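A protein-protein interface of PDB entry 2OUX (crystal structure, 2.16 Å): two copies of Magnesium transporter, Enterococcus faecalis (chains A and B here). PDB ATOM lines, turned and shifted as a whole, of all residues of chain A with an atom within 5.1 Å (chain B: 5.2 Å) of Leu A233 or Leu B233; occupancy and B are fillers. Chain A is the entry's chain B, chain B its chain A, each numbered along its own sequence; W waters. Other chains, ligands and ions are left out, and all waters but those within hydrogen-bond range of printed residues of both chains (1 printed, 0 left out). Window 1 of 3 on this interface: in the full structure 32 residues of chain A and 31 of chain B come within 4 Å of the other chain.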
ATOM      1  N   TYR A 174     -13.523  21.547  -3.292  1.00  0.00           N
ATOM      2  CA  TYR A 174     -13.291  20.117  -3.428  1.00  0.00           C
ATOM      3  C   TYR A 174     -12.261  19.723  -4.481  1.00  0.00           C
ATOM      4  O   TYR A 174     -11.709  18.617  -4.447  1.00  0.00           O
ATOM      5  CB  TYR A 174     -14.626  19.407  -3.615  1.00  0.00           C
ATOM      6  CG  TYR A 174     -15.517  19.603  -2.404  1.00  0.00           C
ATOM      7  CD1 TYR A 174     -14.964  19.712  -1.128  1.00  0.00           C
ATOM      8  CD2 TYR A 174     -16.910  19.667  -2.525  1.00  0.00           C
ATOM      9  CE1 TYR A 174     -15.768  19.878  -0.002  1.00  0.00           C
ATOM     10  CE2 TYR A 174     -17.728  19.836  -1.402  1.00  0.00           C
ATOM     11  CZ  TYR A 174     -17.143  19.938  -0.139  1.00  0.00           C
ATOM     12  OH  TYR A 174     -17.929  20.072   0.983  1.00  0.00           O
ATOM     13  N   TYR A 175     -12.008  20.621  -5.424  1.00  0.00           N
ATOM     14  CA  TYR A 175     -10.962  20.398  -6.411  1.00  0.00           C
ATOM     15  C   TYR A 175     -10.120  21.656  -6.249  1.00  0.00           C
ATOM     16  O   TYR A 175     -10.656  22.772  -6.247  1.00  0.00           O
ATOM     17  CB  TYR A 175     -11.487  20.311  -7.854  1.00  0.00           C
ATOM     18  CG  TYR A 175     -12.230  19.033  -8.216  1.00  0.00           C
ATOM     19  CD1 TYR A 175     -11.843  17.802  -7.701  1.00  0.00           C
ATOM     20  CD2 TYR A 175     -13.289  19.060  -9.117  1.00  0.00           C
ATOM     21  CE1 TYR A 175     -12.504  16.621  -8.074  1.00  0.00           C
ATOM     22  CE2 TYR A 175     -13.950  17.892  -9.497  1.00  0.00           C
ATOM     23  CZ  TYR A 175     -13.555  16.679  -8.975  1.00  0.00           C
ATOM     24  OH  TYR A 175     -14.228  15.537  -9.348  1.00  0.00           O
ATOM     25  N   ILE A 227     -17.745  16.454 -18.432  1.00  0.00           N
ATOM     26  CA  ILE A 227     -18.134  16.307 -17.038  1.00  0.00           C
ATOM     27  C   ILE A 227     -18.868  14.976 -16.836  1.00  0.00           C
ATOM     28  O   ILE A 227     -18.758  14.339 -15.787  1.00  0.00           O
ATOM     29  CB  ILE A 227     -19.042  17.492 -16.582  1.00  0.00           C
ATOM     30  CG1 ILE A 227     -18.190  18.720 -16.229  1.00  0.00           C
ATOM     31  CG2 ILE A 227     -19.896  17.047 -15.400  1.00  0.00           C
ATOM     32  CD1 ILE A 227     -17.343  18.524 -14.977  1.00  0.00           C
ATOM     33  N   ASP A 231     -16.932  12.114 -14.623  1.00  0.00           N
ATOM     34  CA  ASP A 231     -17.660  12.250 -13.359  1.00  0.00           C
ATOM     35  C   ASP A 231     -17.085  13.368 -12.477  1.00  0.00           C
ATOM     36  O   ASP A 231     -16.839  13.164 -11.284  1.00  0.00           O
ATOM     37  CB  ASP A 231     -17.644  10.927 -12.592  1.00  0.00           C
ATOM     38  CG  ASP A 231     -18.316   9.827 -13.355  1.00  0.00           C
ATOM     39  OD1 ASP A 231     -19.252  10.172 -14.076  1.00  0.00           O
ATOM     40  OD2 ASP A 231     -17.933   8.638 -13.244  1.00  0.00           O
ATOM     41  N   PHE A 232     -16.880  14.548 -13.068  1.00  0.00           N
ATOM     42  CA  PHE A 232     -16.315  15.678 -12.337  1.00  0.00           C
ATOM     43  C   PHE A 232     -17.359  16.542 -11.655  1.00  0.00           C
ATOM     44  O   PHE A 232     -18.464  16.702 -12.165  1.00  0.00           O
ATOM     45  CB  PHE A 232     -15.515  16.599 -13.271  1.00  0.00           C
ATOM     46  CG  PHE A 232     -14.227  16.010 -13.780  1.00  0.00           C
ATOM     47  CD1 PHE A 232     -13.453  15.182 -12.975  1.00  0.00           C
ATOM     48  CD2 PHE A 232     -13.738  16.371 -15.041  1.00  0.00           C
ATOM     49  CE1 PHE A 232     -12.214  14.727 -13.412  1.00  0.00           C
ATOM     50  CE2 PHE A 232     -12.504  15.926 -15.482  1.00  0.00           C
ATOM     51  CZ  PHE A 232     -11.737  15.103 -14.665  1.00  0.00           C
ATOM     52  N   LEU A 233     -16.985  17.117 -10.514  1.00  0.00           N
ATOM     53  CA  LEU A 233     -17.857  18.016  -9.777  1.00  0.00           C
ATOM     54  C   LEU A 233     -17.669  19.361 -10.436  1.00  0.00           C
ATOM     55  O   LEU A 233     -18.545  20.214 -10.387  1.00  0.00           O
ATOM     56  CB  LEU A 233     -17.435  18.132  -8.315  1.00  0.00           C
ATOM     57  CG  LEU A 233     -17.462  16.884  -7.438  1.00  0.00           C
ATOM     58  CD1 LEU A 233     -16.901  17.207  -6.061  1.00  0.00           C
ATOM     59  CD2 LEU A 233     -18.886  16.365  -7.344  1.00  0.00           C
ATOM     60  N   ALA A 234     -16.500  19.547 -11.041  1.00  0.00           N
ATOM     61  CA  ALA A 234     -16.169  20.790 -11.728  1.00  0.00           C
ATOM     62  C   ALA A 234     -15.051  20.543 -12.731  1.00  0.00           C
ATOM     63  O   ALA A 234     -14.359  19.541 -12.657  1.00  0.00           O
ATOM     64  CB  ALA A 234     -15.731  21.856 -10.727  1.00  0.00           C
ATOM     65  N   VAL A 235     -14.887  21.470 -13.667  1.00  0.00           N
ATOM     66  CA  VAL A 235     -13.841  21.370 -14.667  1.00  0.00           C
ATOM     67  C   VAL A 235     -13.257  22.765 -14.914  1.00  0.00           C
ATOM     68  O   VAL A 235     -13.990  23.733 -15.047  1.00  0.00           O
ATOM     69  CB  VAL A 235     -14.382  20.775 -15.983  1.00  0.00           C
ATOM     70  CG1 VAL A 235     -15.410  21.714 -16.601  1.00  0.00           C
ATOM     71  CG2 VAL A 235     -13.231  20.505 -16.939  1.00  0.00           C
ATOM     72  N   VAL A 248     -16.308  25.369 -14.484  1.00  0.00           N
ATOM     73  CA  VAL A 248     -17.694  25.078 -14.823  1.00  0.00           C
ATOM     74  C   VAL A 248     -18.096  23.964 -13.875  1.00  0.00           C
ATOM     75  O   VAL A 248     -17.489  22.903 -13.888  1.00  0.00           O
ATOM     76  CB  VAL A 248     -17.821  24.602 -16.275  1.00  0.00           C
ATOM     77  CG1 VAL A 248     -19.217  24.096 -16.542  1.00  0.00           C
ATOM     78  CG2 VAL A 248     -17.481  25.756 -17.211  1.00  0.00           C
ATOM     79  N   THR A 249     -19.107  24.213 -13.051  1.00  0.00           N
ATOM     80  CA  THR A 249     -19.545  23.233 -12.059  1.00  0.00           C
ATOM     81  C   THR A 249     -20.688  22.345 -12.507  1.00  0.00           C
ATOM     82  O   THR A 249     -21.517  22.742 -13.323  1.00  0.00           O
ATOM     83  CB  THR A 249     -19.920  23.928 -10.719  1.00  0.00           C
ATOM     84  OG1 THR A 249     -21.077  24.763 -10.896  1.00  0.00           O
ATOM     85  CG2 THR A 249     -18.759  24.784 -10.249  1.00  0.00           C
ATOM     86  N   VAL A 250     -20.738  21.147 -11.932  1.00  0.00           N
ATOM     87  CA  VAL A 250     -21.740  20.152 -12.286  1.00  0.00           C
ATOM     88  C   VAL A 250     -23.198  20.594 -12.126  1.00  0.00           C
ATOM     89  O   VAL A 250     -24.043  20.252 -12.954  1.00  0.00           O
ATOM     90  CB  VAL A 250     -21.486  18.826 -11.499  1.00  0.00           C
ATOM     91  CG1 VAL A 250     -21.798  19.002 -10.002  1.00  0.00           C
ATOM     92  CG2 VAL A 250     -22.275  17.701 -12.114  1.00  0.00           C
ATOM     93  N   THR B 172     -18.029   9.098  -1.546  1.00  0.00           N
ATOM     94  CA  THR B 172     -17.673  10.490  -1.345  1.00  0.00           C
ATOM     95  C   THR B 172     -17.632  10.788   0.147  1.00  0.00           C
ATOM     96  O   THR B 172     -18.327  10.153   0.937  1.00  0.00           O
ATOM     97  CB  THR B 172     -18.708  11.424  -1.987  1.00  0.00           C
ATOM     98  OG1 THR B 172     -18.241  12.773  -1.911  1.00  0.00           O
ATOM     99  CG2 THR B 172     -20.048  11.312  -1.263  1.00  0.00           C
ATOM    100  N   TYR B 174     -17.469  14.208   0.864  1.00  0.00           N
ATOM    101  CA  TYR B 174     -17.779  15.630   0.839  1.00  0.00           C
ATOM    102  C   TYR B 174     -19.014  16.010   1.627  1.00  0.00           C
ATOM    103  O   TYR B 174     -19.298  17.183   1.838  1.00  0.00           O
ATOM    104  CB  TYR B 174     -17.822  16.132  -0.606  1.00  0.00           C
ATOM    105  CG  TYR B 174     -16.433  16.040  -1.229  1.00  0.00           C
ATOM    106  CD1 TYR B 174     -15.296  16.220  -0.440  1.00  0.00           C
ATOM    107  CD2 TYR B 174     -16.255  15.730  -2.573  1.00  0.00           C
ATOM    108  CE1 TYR B 174     -14.009  16.081  -0.970  1.00  0.00           C
ATOM    109  CE2 TYR B 174     -14.970  15.590  -3.119  1.00  0.00           C
ATOM    110  CZ  TYR B 174     -13.850  15.767  -2.305  1.00  0.00           C
ATOM    111  OH  TYR B 174     -12.581  15.612  -2.819  1.00  0.00           O
ATOM    112  N   TYR B 175     -19.742  14.995   2.068  1.00  0.00           N
ATOM    113  CA  TYR B 175     -20.900  15.192   2.923  1.00  0.00           C
ATOM    114  C   TYR B 175     -20.715  14.130   3.987  1.00  0.00           C
ATOM    115  O   TYR B 175     -20.383  12.987   3.672  1.00  0.00           O
ATOM    116  CB  TYR B 175     -22.222  14.951   2.181  1.00  0.00           C
ATOM    117  CG  TYR B 175     -22.714  16.133   1.388  1.00  0.00           C
ATOM    118  CD1 TYR B 175     -22.874  17.372   1.995  1.00  0.00           C
ATOM    119  CD2 TYR B 175     -23.013  16.019   0.032  1.00  0.00           C
ATOM    120  CE1 TYR B 175     -23.320  18.469   1.276  1.00  0.00           C
ATOM    121  CE2 TYR B 175     -23.457  17.110  -0.698  1.00  0.00           C
ATOM    122  CZ  TYR B 175     -23.606  18.331  -0.072  1.00  0.00           C
ATOM    123  OH  TYR B 175     -24.034  19.426  -0.784  1.00  0.00           O
ATOM    124  N   ASP B 231     -28.823  21.647  -5.745  1.00  0.00           N
ATOM    125  CA  ASP B 231     -27.442  21.661  -6.229  1.00  0.00           C
ATOM    126  C   ASP B 231     -26.522  20.805  -5.340  1.00  0.00           C
ATOM    127  O   ASP B 231     -25.416  21.219  -4.996  1.00  0.00           O
ATOM    128  CB  ASP B 231     -26.923  23.105  -6.289  1.00  0.00           C
ATOM    129  CG  ASP B 231     -27.758  23.989  -7.209  1.00  0.00           C
ATOM    130  OD1 ASP B 231     -28.248  23.470  -8.220  1.00  0.00           O
ATOM    131  OD2 ASP B 231     -27.916  25.196  -6.936  1.00  0.00           O
ATOM    132  N   PHE B 232     -26.990  19.618  -4.956  1.00  0.00           N
ATOM    133  CA  PHE B 232     -26.203  18.715  -4.117  1.00  0.00           C
ATOM    134  C   PHE B 232     -25.392  17.763  -4.991  1.00  0.00           C
ATOM    135  O   PHE B 232     -25.814  17.429  -6.102  1.00  0.00           O
ATOM    136  CB  PHE B 232     -27.098  17.846  -3.242  1.00  0.00           C
ATOM    137  CG  PHE B 232     -27.800  18.579  -2.143  1.00  0.00           C
ATOM    138  CD1 PHE B 232     -27.209  19.660  -1.511  1.00  0.00           C
ATOM    139  CD2 PHE B 232     -29.021  18.112  -1.666  1.00  0.00           C
ATOM    140  CE1 PHE B 232     -27.819  20.260  -0.410  1.00  0.00           C
ATOM    141  CE2 PHE B 232     -29.631  18.706  -0.569  1.00  0.00           C
ATOM    142  CZ  PHE B 232     -29.028  19.779   0.058  1.00  0.00           C
ATOM    143  N   LEU B 233     -24.245  17.314  -4.484  1.00  0.00           N
ATOM    144  CA  LEU B 233     -23.412  16.374  -5.228  1.00  0.00           C
ATOM    145  C   LEU B 233     -23.793  14.966  -4.781  1.00  0.00           C
ATOM    146  O   LEU B 233     -23.330  13.971  -5.333  1.00  0.00           O
ATOM    147  CB  LEU B 233     -21.928  16.663  -4.979  1.00  0.00           C
ATOM    148  CG  LEU B 233     -21.427  16.648  -3.534  1.00  0.00           C
ATOM    149  CD1 LEU B 233     -21.091  15.212  -3.114  1.00  0.00           C
ATOM    150  CD2 LEU B 233     -20.187  17.531  -3.431  1.00  0.00           C
ATOM    151  N   ALA B 234     -24.656  14.897  -3.773  1.00  0.00           N
ATOM    152  CA  ALA B 234     -25.145  13.621  -3.262  1.00  0.00           C
ATOM    153  C   ALA B 234     -26.357  13.862  -2.367  1.00  0.00           C
ATOM    154  O   ALA B 234     -26.544  14.967  -1.852  1.00  0.00           O
ATOM    155  CB  ALA B 234     -24.047  12.894  -2.478  1.00  0.00           C
ATOM    156  N   VAL B 235     -27.186  12.834  -2.198  1.00  0.00           N
ATOM    157  CA  VAL B 235     -28.361  12.940  -1.351  1.00  0.00           C
ATOM    158  C   VAL B 235     -28.620  11.614  -0.655  1.00  0.00           C
ATOM    159  O   VAL B 235     -28.613  10.558  -1.284  1.00  0.00           O
ATOM    160  CB  VAL B 235     -29.611  13.396  -2.161  1.00  0.00           C
ATOM    161  CG1 VAL B 235     -30.045  12.320  -3.153  1.00  0.00           C
ATOM    162  CG2 VAL B 235     -30.736  13.761  -1.202  1.00  0.00           C
ATOM    163  N   VAL B 248     -27.308   8.785  -3.305  1.00  0.00           N
ATOM    164  CA  VAL B 248     -27.416   8.846  -4.752  1.00  0.00           C
ATOM    165  C   VAL B 248     -26.539  10.038  -5.121  1.00  0.00           C
ATOM    166  O   VAL B 248     -26.751  11.140  -4.625  1.00  0.00           O
ATOM    167  CB  VAL B 248     -28.874   9.090  -5.186  1.00  0.00           C
ATOM    168  CG1 VAL B 248     -28.935   9.437  -6.637  1.00  0.00           C
ATOM    169  CG2 VAL B 248     -29.701   7.854  -4.921  1.00  0.00           C
ATOM    170  N   THR B 249     -25.560   9.807  -5.991  1.00  0.00           N
ATOM    171  CA  THR B 249     -24.619  10.839  -6.394  1.00  0.00           C
ATOM    172  C   THR B 249     -24.974  11.560  -7.686  1.00  0.00           C
ATOM    173  O   THR B 249     -25.613  10.995  -8.562  1.00  0.00           O
ATOM    174  CB  THR B 249     -23.212  10.234  -6.508  1.00  0.00           C
ATOM    175  OG1 THR B 249     -23.235   9.130  -7.424  1.00  0.00           O
ATOM    176  CG2 THR B 249     -22.763   9.728  -5.152  1.00  0.00           C
ATOM    177  N   VAL B 250     -24.530  12.811  -7.806  1.00  0.00           N
ATOM    178  CA  VAL B 250     -24.847  13.606  -8.981  1.00  0.00           C
ATOM    179  C   VAL B 250     -24.389  13.008 -10.307  1.00  0.00           C
ATOM    180  O   VAL B 250     -25.027  13.219 -11.333  1.00  0.00           O
ATOM    181  CB  VAL B 250     -24.284  15.049  -8.871  1.00  0.00           C
ATOM    182  CG1 VAL B 250     -22.754  15.050  -8.970  1.00  0.00           C
ATOM    183  CG2 VAL B 250     -24.885  15.913  -9.950  1.00  0.00           C
HETATM  184  O   HOH W   1     -20.514  19.657   0.173  1.00  0.00           O
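Of the 11 printed residues of chain B, 3 touch a printed residue of chain A.
Hydrophobic or aromatic side chains of chain B that line the printed part of chain A: Tyr B174, Leu B233 and Val B250.
Of the 11 printed residues of chain A, 3 touch a printed residue of chain B.
Among the printed residues, no Asp or Glu carboxylate lies within 4 Å of a Lys or Arg side-chain nitrogen of the other chain.
O of Tyr B174 lies within hydrogen-bond range of OH of Tyr A174, 3.3 Å away.
N of Leu A233 lies close to OH of Tyr A175 (3.4 Å).
The backbone carbonyl oxygen of Leu B233 is in hydrogen-bond range of the backbone NH of Val B250, 3.0 Å away.
The backbone NH (N) of Tyr B174 is in hydrogen-bond range of the side-chain hydroxyl (OG1) of Thr B172, 3.2 Å away.
The backbone carbonyl oxygen of Leu A233 lies within hydrogen-bond range of the backbone NH of Val A250 (2.8 Å).
Tyr B174 touches its own counterpart, Tyr A174.
Tyr A174 touches Leu B233, and with the chains exchanged Leu A233 touches Tyr B174.
Leu A233 touches its own counterpart, Leu B233.
Val A250 touches its own counterpart, Val B250.
Positions printed for both chains: 174, 175, 231, 232, 233, 234, 235, 248, 249 and 250.
Water W1 bridges OH of Tyr A174 (2.7 Å) and O of Tyr B174 (3.2 Å).
Among the printed residues, pairs that only touch across the chains: Val A250 with Val B250 (3.8 Å), Leu A233 with Tyr B174 (3.8 Å), Leu A233 with Leu B233 (3.9 Å) and Tyr A174 with Leu B233 (3.9 Å).
Of chain B, only Tyr B174 and Leu B233 come within 4 Å of Leu A233.
Leu B233 touches just these residues of chain A: Tyr A174 (3.9 Å) and Leu A233 (3.9 Å).
Of the printed residues of chain A, Tyr B174 touches Tyr A174 (3.3 Å) and Leu A233 (3.8 Å).
Printed residues of chain B within 4 Å of Tyr A174: Tyr B174 and Leu B233.
Printed residues of chain A within 4 Å of Val B250: Val A250.
Of the printed residues of chain B, Val A250 touches Val B250.
Asp A231 touches none of the printed residues of chain B.
Thr A249 touches none of the printed residues of chain B.
The nearest printed residue of chain B that does not touch Tyr A174 is Tyr B175 (5.5 Å).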
